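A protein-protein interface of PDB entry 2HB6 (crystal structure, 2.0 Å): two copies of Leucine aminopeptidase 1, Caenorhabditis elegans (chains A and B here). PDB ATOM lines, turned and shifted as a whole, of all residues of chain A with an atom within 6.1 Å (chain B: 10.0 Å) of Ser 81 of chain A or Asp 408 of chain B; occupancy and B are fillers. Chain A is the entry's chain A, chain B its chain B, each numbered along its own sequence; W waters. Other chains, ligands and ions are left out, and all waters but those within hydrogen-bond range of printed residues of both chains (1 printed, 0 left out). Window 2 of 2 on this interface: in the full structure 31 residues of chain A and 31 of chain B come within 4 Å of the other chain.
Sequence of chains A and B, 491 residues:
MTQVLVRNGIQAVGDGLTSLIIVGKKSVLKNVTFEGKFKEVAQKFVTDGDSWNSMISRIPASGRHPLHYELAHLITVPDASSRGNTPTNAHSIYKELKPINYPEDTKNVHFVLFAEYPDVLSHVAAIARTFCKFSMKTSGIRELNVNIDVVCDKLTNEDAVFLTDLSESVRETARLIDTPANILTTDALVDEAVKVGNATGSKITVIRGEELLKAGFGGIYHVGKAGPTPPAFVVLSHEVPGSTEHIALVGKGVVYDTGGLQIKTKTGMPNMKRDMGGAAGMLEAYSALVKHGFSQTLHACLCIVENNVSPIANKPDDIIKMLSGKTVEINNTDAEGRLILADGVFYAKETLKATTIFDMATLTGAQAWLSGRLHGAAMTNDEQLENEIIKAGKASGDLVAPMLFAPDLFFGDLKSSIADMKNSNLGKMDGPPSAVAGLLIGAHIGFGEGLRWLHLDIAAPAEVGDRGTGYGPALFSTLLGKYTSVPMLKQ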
ATOM      1  N   ASP A  79      -0.174  14.590  23.349  1.00  0.00           N
ATOM      2  CA  ASP A  79       0.317  14.996  22.032  1.00  0.00           C
ATOM      3  C   ASP A  79       1.381  14.051  21.471  1.00  0.00           C
ATOM      4  O   ASP A  79       1.380  13.758  20.283  1.00  0.00           O
ATOM      5  CB  ASP A  79       0.848  16.429  22.072  1.00  0.00           C
ATOM      6  CG  ASP A  79      -0.271  17.455  22.067  1.00  0.00           C
ATOM      7  OD1 ASP A  79      -0.941  17.603  21.023  1.00  0.00           O
ATOM      8  OD2 ASP A  79      -0.486  18.093  23.109  1.00  0.00           O
ATOM      9  N   ALA A  80       2.283  13.591  22.335  1.00  0.00           N
ATOM     10  CA  ALA A  80       3.417  12.775  21.913  1.00  0.00           C
ATOM     11  C   ALA A  80       2.981  11.326  21.679  1.00  0.00           C
ATOM     12  O   ALA A  80       2.075  10.834  22.355  1.00  0.00           O
ATOM     13  CB  ALA A  80       4.512  12.829  22.974  1.00  0.00           C
ATOM     14  N   SER A  81       3.627  10.648  20.729  1.00  0.00           N
ATOM     15  CA  SER A  81       3.395   9.216  20.507  1.00  0.00           C
ATOM     16  C   SER A  81       4.629   8.572  19.915  1.00  0.00           C
ATOM     17  O   SER A  81       5.379   9.215  19.179  1.00  0.00           O
ATOM     18  CB  SER A  81       2.229   8.978  19.541  1.00  0.00           C
ATOM     19  OG  SER A  81       2.501   9.588  18.296  1.00  0.00           O
ATOM     20  N   SER A  82       4.814   7.291  20.220  1.00  0.00           N
ATOM     21  CA  SER A  82       5.912   6.511  19.664  1.00  0.00           C
ATOM     22  C   SER A  82       5.577   6.090  18.251  1.00  0.00           C
ATOM     23  O   SER A  82       4.405   6.121  17.818  1.00  0.00           O
ATOM     24  CB  SER A  82       6.145   5.252  20.510  1.00  0.00           C
ATOM     25  OG  SER A  82       5.004   4.411  20.422  1.00  0.00           O
ATOM     26  N   ARG A  83       6.600   5.641  17.539  1.00  0.00           N
ATOM     27  CA  ARG A  83       6.432   5.230  16.161  1.00  0.00           C
ATOM     28  C   ARG A  83       5.557   3.977  15.972  1.00  0.00           C
ATOM     29  O   ARG A  83       4.910   3.849  14.946  1.00  0.00           O
ATOM     30  CB  ARG A  83       7.781   5.079  15.467  1.00  0.00           C
ATOM     31  CG  ARG A  83       8.688   4.039  16.072  1.00  0.00           C
ATOM     32  CD  ARG A  83      10.069   4.118  15.422  1.00  0.00           C
ATOM     33  NE  ARG A  83      10.749   2.834  15.487  1.00  0.00           N
ATOM     34  CZ  ARG A  83      10.610   1.865  14.592  1.00  0.00           C
ATOM     35  NH1 ARG A  83      11.272   0.725  14.748  1.00  0.00           N
ATOM     36  NH2 ARG A  83       9.819   2.034  13.538  1.00  0.00           N
ATOM     37  N   GLY A  84       5.509   3.090  16.965  1.00  0.00           N
ATOM     38  CA  GLY A  84       4.635   1.897  16.905  1.00  0.00           C
ATOM     39  C   GLY A  84       3.165   2.145  17.248  1.00  0.00           C
ATOM     40  O   GLY A  84       2.285   1.313  16.945  1.00  0.00           O
ATOM     41  N   ASN A  85       2.902   3.299  17.842  1.00  0.00           N
ATOM     42  CA  ASN A  85       1.571   3.721  18.234  1.00  0.00           C
ATOM     43  C   ASN A  85       0.931   4.513  17.100  1.00  0.00           C
ATOM     44  O   ASN A  85       1.546   4.738  16.070  1.00  0.00           O
ATOM     45  CB  ASN A  85       1.707   4.649  19.439  1.00  0.00           C
ATOM     46  CG  ASN A  85       0.400   4.870  20.183  1.00  0.00           C
ATOM     47  OD1 ASN A  85      -0.637   4.357  19.811  1.00  0.00           O
ATOM     48  ND2 ASN A  85       0.466   5.639  21.247  1.00  0.00           N
ATOM     49  N   THR A  86      -0.299   4.948  17.308  1.00  0.00           N
ATOM     50  CA  THR A  86      -0.974   5.791  16.354  1.00  0.00           C
ATOM     51  C   THR A  86      -0.750   7.198  16.894  1.00  0.00           C
ATOM     52  O   THR A  86      -0.848   7.412  18.077  1.00  0.00           O
ATOM     53  CB  THR A  86      -2.485   5.496  16.283  1.00  0.00           C
ATOM     54  OG1 THR A  86      -3.160   6.634  15.753  1.00  0.00           O
ATOM     55  CG2 THR A  86      -3.084   5.341  17.663  1.00  0.00           C
ATOM     56  N   PRO A  87      -0.410   8.146  16.035  1.00  0.00           N
ATOM     57  CA  PRO A  87      -0.209   9.516  16.503  1.00  0.00           C
ATOM     58  C   PRO A  87      -1.503  10.212  16.943  1.00  0.00           C
ATOM     59  O   PRO A  87      -1.443  11.252  17.601  1.00  0.00           O
ATOM     60  CB  PRO A  87       0.401  10.227  15.284  1.00  0.00           C
ATOM     61  CG  PRO A  87      -0.099   9.458  14.114  1.00  0.00           C
ATOM     62  CD  PRO A  87      -0.221   8.028  14.575  1.00  0.00           C
ATOM     63  N   THR A  88      -2.651   9.614  16.619  1.00  0.00           N
ATOM     64  CA  THR A  88      -3.937  10.067  17.163  1.00  0.00           C
ATOM     65  C   THR A  88      -4.042   9.859  18.669  1.00  0.00           C
ATOM     66  O   THR A  88      -4.827  10.544  19.338  1.00  0.00           O
ATOM     67  CB  THR A  88      -5.139   9.352  16.497  1.00  0.00           C
ATOM     68  OG1 THR A  88      -5.212   8.003  16.961  1.00  0.00           O
ATOM     69  CG2 THR A  88      -5.029   9.357  14.964  1.00  0.00           C
ATOM     70  N   ASN A  89      -3.349   8.846  19.196  1.00  0.00           N
ATOM     71  CA  ASN A  89      -3.424   8.465  20.617  1.00  0.00           C
ATOM     72  C   ASN A  89      -4.898   8.165  21.005  1.00  0.00           C
ATOM     73  O   ASN A  89      -5.322   8.427  22.111  1.00  0.00           O
ATOM     74  CB  ASN A  89      -2.877   9.584  21.506  1.00  0.00           C
ATOM     75  CG  ASN A  89      -1.354   9.579  21.615  1.00  0.00           C
ATOM     76  OD1 ASN A  89      -0.730  10.621  21.627  1.00  0.00           O
ATOM     77  ND2 ASN A  89      -0.773   8.408  21.720  1.00  0.00           N
ATOM     78  N   MET B 379      14.068  -4.745  18.132  1.00  0.00           N
ATOM     79  CA  MET B 379      13.284  -3.590  18.561  1.00  0.00           C
ATOM     80  C   MET B 379      14.192  -2.373  18.625  1.00  0.00           C
ATOM     81  O   MET B 379      15.188  -2.375  19.356  1.00  0.00           O
ATOM     82  CB  MET B 379      12.691  -3.852  19.944  1.00  0.00           C
ATOM     83  CG  MET B 379      11.605  -2.866  20.382  1.00  0.00           C
ATOM     84  SD  MET B 379      11.059  -3.200  22.073  1.00  0.00           S
ATOM     85  CE  MET B 379      12.435  -2.497  22.980  1.00  0.00           C
ATOM     86  N   ASN B 381      14.421   2.232  18.315  1.00  0.00           N
ATOM     87  CA  ASN B 381      13.826   3.569  18.220  1.00  0.00           C
ATOM     88  C   ASN B 381      14.019   4.220  16.842  1.00  0.00           C
ATOM     89  O   ASN B 381      13.465   5.285  16.562  1.00  0.00           O
ATOM     90  CB  ASN B 381      14.360   4.484  19.329  1.00  0.00           C
ATOM     91  CG  ASN B 381      15.835   4.826  19.158  1.00  0.00           C
ATOM     92  OD1 ASN B 381      16.631   3.995  18.727  1.00  0.00           O
ATOM     93  ND2 ASN B 381      16.203   6.049  19.506  1.00  0.00           N
ATOM     94  N   LEU B 404       7.483  -4.456  17.331  1.00  0.00           N
ATOM     95  CA  LEU B 404       6.922  -3.137  17.659  1.00  0.00           C
ATOM     96  C   LEU B 404       7.756  -2.360  18.664  1.00  0.00           C
ATOM     97  O   LEU B 404       8.155  -2.892  19.717  1.00  0.00           O
ATOM     98  CB  LEU B 404       5.477  -3.249  18.197  1.00  0.00           C
ATOM     99  CG  LEU B 404       4.370  -3.585  17.200  1.00  0.00           C
ATOM    100  CD1 LEU B 404       3.081  -3.924  17.963  1.00  0.00           C
ATOM    101  CD2 LEU B 404       4.132  -2.430  16.199  1.00  0.00           C
ATOM    102  N   PHE B 405       7.971  -1.085  18.349  1.00  0.00           N
ATOM    103  CA  PHE B 405       8.555  -0.144  19.281  1.00  0.00           C
ATOM    104  C   PHE B 405       7.484   0.834  19.779  1.00  0.00           C
ATOM    105  O   PHE B 405       7.112   1.772  19.067  1.00  0.00           O
ATOM    106  CB  PHE B 405       9.690   0.640  18.603  1.00  0.00           C
ATOM    107  CG  PHE B 405      10.429   1.562  19.544  1.00  0.00           C
ATOM    108  CD1 PHE B 405      11.433   1.074  20.371  1.00  0.00           C
ATOM    109  CD2 PHE B 405      10.116   2.914  19.611  1.00  0.00           C
ATOM    110  CE1 PHE B 405      12.101   1.921  21.249  1.00  0.00           C
ATOM    111  CE2 PHE B 405      10.785   3.760  20.486  1.00  0.00           C
ATOM    112  CZ  PHE B 405      11.773   3.260  21.301  1.00  0.00           C
ATOM    113  N   ALA B 406       7.004   0.627  21.002  1.00  0.00           N
ATOM    114  CA  ALA B 406       6.018   1.544  21.571  1.00  0.00           C
ATOM    115  C   ALA B 406       6.118   1.643  23.092  1.00  0.00           C
ATOM    116  O   ALA B 406       5.279   1.091  23.793  1.00  0.00           O
ATOM    117  CB  ALA B 406       4.603   1.127  21.145  1.00  0.00           C
ATOM    118  N   PRO B 407       7.132   2.371  23.606  1.00  0.00           N
ATOM    119  CA  PRO B 407       7.243   2.488  25.060  1.00  0.00           C
ATOM    120  C   PRO B 407       5.976   3.108  25.666  1.00  0.00           C
ATOM    121  O   PRO B 407       5.542   2.678  26.729  1.00  0.00           O
ATOM    122  CB  PRO B 407       8.444   3.420  25.255  1.00  0.00           C
ATOM    123  CG  PRO B 407       9.251   3.281  23.999  1.00  0.00           C
ATOM    124  CD  PRO B 407       8.202   3.118  22.911  1.00  0.00           C
ATOM    125  N   ASP B 408       5.365   4.068  24.976  1.00  0.00           N
ATOM    126  CA  ASP B 408       4.142   4.692  25.500  1.00  0.00           C
ATOM    127  C   ASP B 408       3.004   3.700  25.741  1.00  0.00           C
ATOM    128  O   ASP B 408       2.325   3.769  26.753  1.00  0.00           O
ATOM    129  CB  ASP B 408       3.692   5.896  24.647  1.00  0.00           C
ATOM    130  CG  ASP B 408       3.539   5.564  23.171  1.00  0.00           C
ATOM    131  OD1 ASP B 408       3.869   4.429  22.735  1.00  0.00           O
ATOM    132  OD2 ASP B 408       3.098   6.464  22.427  1.00  0.00           O
ATOM    133  N   LEU B 409       2.817   2.765  24.819  1.00  0.00           N
ATOM    134  CA  LEU B 409       1.775   1.743  24.945  1.00  0.00           C
ATOM    135  C   LEU B 409       2.141   0.607  25.905  1.00  0.00           C
ATOM    136  O   LEU B 409       1.265   0.051  26.563  1.00  0.00           O
ATOM    137  CB  LEU B 409       1.443   1.161  23.569  1.00  0.00           C
ATOM    138  CG  LEU B 409       0.806   2.121  22.553  1.00  0.00           C
ATOM    139  CD1 LEU B 409       0.520   1.360  21.262  1.00  0.00           C
ATOM    140  CD2 LEU B 409      -0.501   2.769  23.115  1.00  0.00           C
ATOM    141  N   PHE B 410       3.422   0.229  25.952  1.00  0.00           N
ATOM    142  CA  PHE B 410       3.802  -1.042  26.586  1.00  0.00           C
ATOM    143  C   PHE B 410       4.593  -0.921  27.892  1.00  0.00           C
ATOM    144  O   PHE B 410       4.633  -1.868  28.664  1.00  0.00           O
ATOM    145  CB  PHE B 410       4.569  -1.963  25.611  1.00  0.00           C
ATOM    146  CG  PHE B 410       3.867  -2.219  24.283  1.00  0.00           C
ATOM    147  CD1 PHE B 410       2.469  -2.279  24.187  1.00  0.00           C
ATOM    148  CD2 PHE B 410       4.624  -2.445  23.131  1.00  0.00           C
ATOM    149  CE1 PHE B 410       1.848  -2.549  22.953  1.00  0.00           C
ATOM    150  CE2 PHE B 410       4.025  -2.710  21.899  1.00  0.00           C
ATOM    151  CZ  PHE B 410       2.624  -2.763  21.812  1.00  0.00           C
ATOM    152  N   PHE B 411       5.246   0.212  28.142  1.00  0.00           N
ATOM    153  CA  PHE B 411       6.126   0.305  29.324  1.00  0.00           C
ATOM    154  C   PHE B 411       5.316   0.222  30.613  1.00  0.00           C
ATOM    155  O   PHE B 411       5.829  -0.197  31.651  1.00  0.00           O
ATOM    156  CB  PHE B 411       7.000   1.573  29.308  1.00  0.00           C
ATOM    157  CG  PHE B 411       7.936   1.686  30.511  1.00  0.00           C
ATOM    158  CD1 PHE B 411       8.895   0.698  30.759  1.00  0.00           C
ATOM    159  CD2 PHE B 411       7.837   2.762  31.390  1.00  0.00           C
ATOM    160  CE1 PHE B 411       9.744   0.789  31.871  1.00  0.00           C
ATOM    161  CE2 PHE B 411       8.685   2.867  32.494  1.00  0.00           C
ATOM    162  CZ  PHE B 411       9.641   1.879  32.727  1.00  0.00           C
ATOM    163  N   GLY B 412       4.032   0.574  30.528  1.00  0.00           N
ATOM    164  CA  GLY B 412       3.093   0.409  31.655  1.00  0.00           C
ATOM    165  C   GLY B 412       2.931  -1.025  32.159  1.00  0.00           C
ATOM    166  O   GLY B 412       2.542  -1.244  33.315  1.00  0.00           O
ATOM    167  N   ASP B 413       3.251  -2.005  31.312  1.00  0.00           N
ATOM    168  CA  ASP B 413       3.324  -3.404  31.737  1.00  0.00           C
ATOM    169  C   ASP B 413       4.332  -3.641  32.882  1.00  0.00           C
ATOM    170  O   ASP B 413       4.219  -4.622  33.614  1.00  0.00           O
ATOM    171  CB  ASP B 413       3.671  -4.308  30.543  1.00  0.00           C
ATOM    172  CG  ASP B 413       2.587  -4.318  29.472  1.00  0.00           C
ATOM    173  OD1 ASP B 413       1.419  -3.994  29.788  1.00  0.00           O
ATOM    174  OD2 ASP B 413       2.900  -4.682  28.314  1.00  0.00           O
ATOM    175  N   LEU B 414       5.300  -2.741  33.028  1.00  0.00           N
ATOM    176  CA  LEU B 414       6.327  -2.859  34.068  1.00  0.00           C
ATOM    177  C   LEU B 414       6.137  -1.883  35.222  1.00  0.00           C
ATOM    178  O   LEU B 414       7.064  -1.644  35.978  1.00  0.00           O
ATOM    179  CB  LEU B 414       7.719  -2.676  33.466  1.00  0.00           C
ATOM    180  CG  LEU B 414       8.058  -3.636  32.327  1.00  0.00           C
ATOM    181  CD1 LEU B 414       9.407  -3.315  31.725  1.00  0.00           C
ATOM    182  CD2 LEU B 414       8.042  -5.083  32.845  1.00  0.00           C
ATOM    183  N   ASP B 430      -0.036  -5.713  27.813  1.00  0.00           N
ATOM    184  CA  ASP B 430      -0.471  -5.136  26.545  1.00  0.00           C
ATOM    185  C   ASP B 430       0.558  -5.346  25.438  1.00  0.00           C
ATOM    186  O   ASP B 430       0.192  -5.424  24.276  1.00  0.00           O
ATOM    187  CB  ASP B 430      -0.716  -3.631  26.720  1.00  0.00           C
ATOM    188  CG  ASP B 430      -2.060  -3.338  27.357  1.00  0.00           C
ATOM    189  OD1 ASP B 430      -2.909  -4.247  27.388  1.00  0.00           O
ATOM    190  OD2 ASP B 430      -2.267  -2.198  27.809  1.00  0.00           O
ATOM    191  N   GLY B 431       1.839  -5.404  25.789  1.00  0.00           N
ATOM    192  CA  GLY B 431       2.884  -5.569  24.765  1.00  0.00           C
ATOM    193  C   GLY B 431       3.193  -7.018  24.458  1.00  0.00           C
ATOM    194  O   GLY B 431       2.905  -7.896  25.266  1.00  0.00           O
ATOM    195  N   LEU B 439      12.028  -3.404  26.559  1.00  0.00           N
ATOM    196  CA  LEU B 439      11.733  -2.091  27.139  1.00  0.00           C
ATOM    197  C   LEU B 439      12.288  -1.907  28.548  1.00  0.00           C
ATOM    198  O   LEU B 439      12.627  -0.792  28.929  1.00  0.00           O
ATOM    199  CB  LEU B 439      10.224  -1.787  27.117  1.00  0.00           C
ATOM    200  CG  LEU B 439       9.634  -1.577  25.713  1.00  0.00           C
ATOM    201  CD1 LEU B 439       8.109  -1.571  25.826  1.00  0.00           C
ATOM    202  CD2 LEU B 439      10.145  -0.272  25.016  1.00  0.00           C
ATOM    203  N   GLY B 446      16.360   6.026  28.457  1.00  0.00           N
ATOM    204  CA  GLY B 446      15.309   6.849  27.852  1.00  0.00           C
ATOM    205  C   GLY B 446      14.810   6.297  26.531  1.00  0.00           C
ATOM    206  O   GLY B 446      14.458   7.061  25.623  1.00  0.00           O
ATOM    207  N   PHE B 447      14.798   4.966  26.423  1.00  0.00           N
ATOM    208  CA  PHE B 447      14.381   4.242  25.205  1.00  0.00           C
ATOM    209  C   PHE B 447      15.130   4.655  23.932  1.00  0.00           C
ATOM    210  O   PHE B 447      14.593   4.567  22.827  1.00  0.00           O
ATOM    211  CB  PHE B 447      12.849   4.309  25.015  1.00  0.00           C
ATOM    212  CG  PHE B 447      12.078   3.949  26.255  1.00  0.00           C
ATOM    213  CD1 PHE B 447      12.017   2.624  26.687  1.00  0.00           C
ATOM    214  CD2 PHE B 447      11.431   4.931  27.004  1.00  0.00           C
ATOM    215  CE1 PHE B 447      11.305   2.271  27.856  1.00  0.00           C
ATOM    216  CE2 PHE B 447      10.730   4.592  28.179  1.00  0.00           C
ATOM    217  CZ  PHE B 447      10.669   3.254  28.601  1.00  0.00           C
HETATM  218  O   HOH W   1       1.537   8.367  23.709  1.00  0.00           O
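Among the printed residues, merely in contact across the chains: Ser 82 of chain A with Ala 406 of chain B, Ser 81 of chain A with Asp 408 of chain B, Asn 85 of chain A with Leu 409 of chain B, Ser 82 of chain A with Phe 405 of chain B, Arg 83 of chain A with Asn 381 of chain B, Ser 82 of chain A with Pro 407 of chain B and Arg 83 of chain A with Phe 405 of chain B.
Of the 11 printed residues of chain A, 5 touch a printed residue of chain B. Printed residues of chain A that touch a printed residue of chain B: Ser 81, Ser 82, Arg 83, Gly 84 and Asn 85. Among the printed residues, 10 pairs touch across the chains. Among the printed residues, no Asp or Glu carboxylate lies within 4 Å of a Lys or Arg side-chain nitrogen of the other chain.
No position is printed for both chains.
Water W1 lies within hydrogen-bond range of the side-chain carboxylate of Asp 408 of chain B, the backbone carbonyl oxygen of Ala 80 of chain A and the side-chain amide nitrogen of Asn 89 of chain A.
No residue of chain B comes within 4 Å of Ala 80 of chain A. Of chain B, only Asp 408 comes within 4 Å of Ser 81 of chain A. Ser 82 of chain A touches just these residues of chain B: Phe 405, Ala 406, Pro 407 and Asp 408. Of the printed residues of chain B, Arg 83 of chain A touches Asn 381 (3.8 Å) and Phe 405 (3.96 Å). Asn 85 of chain A touches just these residues of chain B: Asp 408 and Leu 409. Of the printed residues of chain A, Asn 381 of chain B touches Arg 83 (3.8 Å). Of the printed residues of chain A, Phe 405 of chain B touches Ser 82, Arg 83 and Gly 84. Printed residues of chain A within 4 Å of Pro 407 of chain B: Ser 82 (3.8 Å). Of chain A, only Ser 81 (3.4 Å), Ser 82 (2.6 Å) and Asn 85 (3.0 Å) come within 4 Å of Asp 408 of chain B. The nearest residue of chain A that does not touch Asp 408 of chain B is Asn 89 of chain A (4.4 Å).
OG of Ser 82 of chain A lies within hydrogen-bond range of OD1 of Asp 408 of chain B, 2.6 Å away. The backbone NH of Gly 84 of chain A is in hydrogen-bond range of the backbone carbonyl oxygen of Phe 405 of chain B (3.0 Å). ND2 of Asn 85 of chain A sits at hydrogen-bond distance from OD2 of Asp 408 of chain B (3.0 Å).
ND2 of Asn 85 of chain A lies close to ND2 of Asn 89 of chain A, at 3.1 Å.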
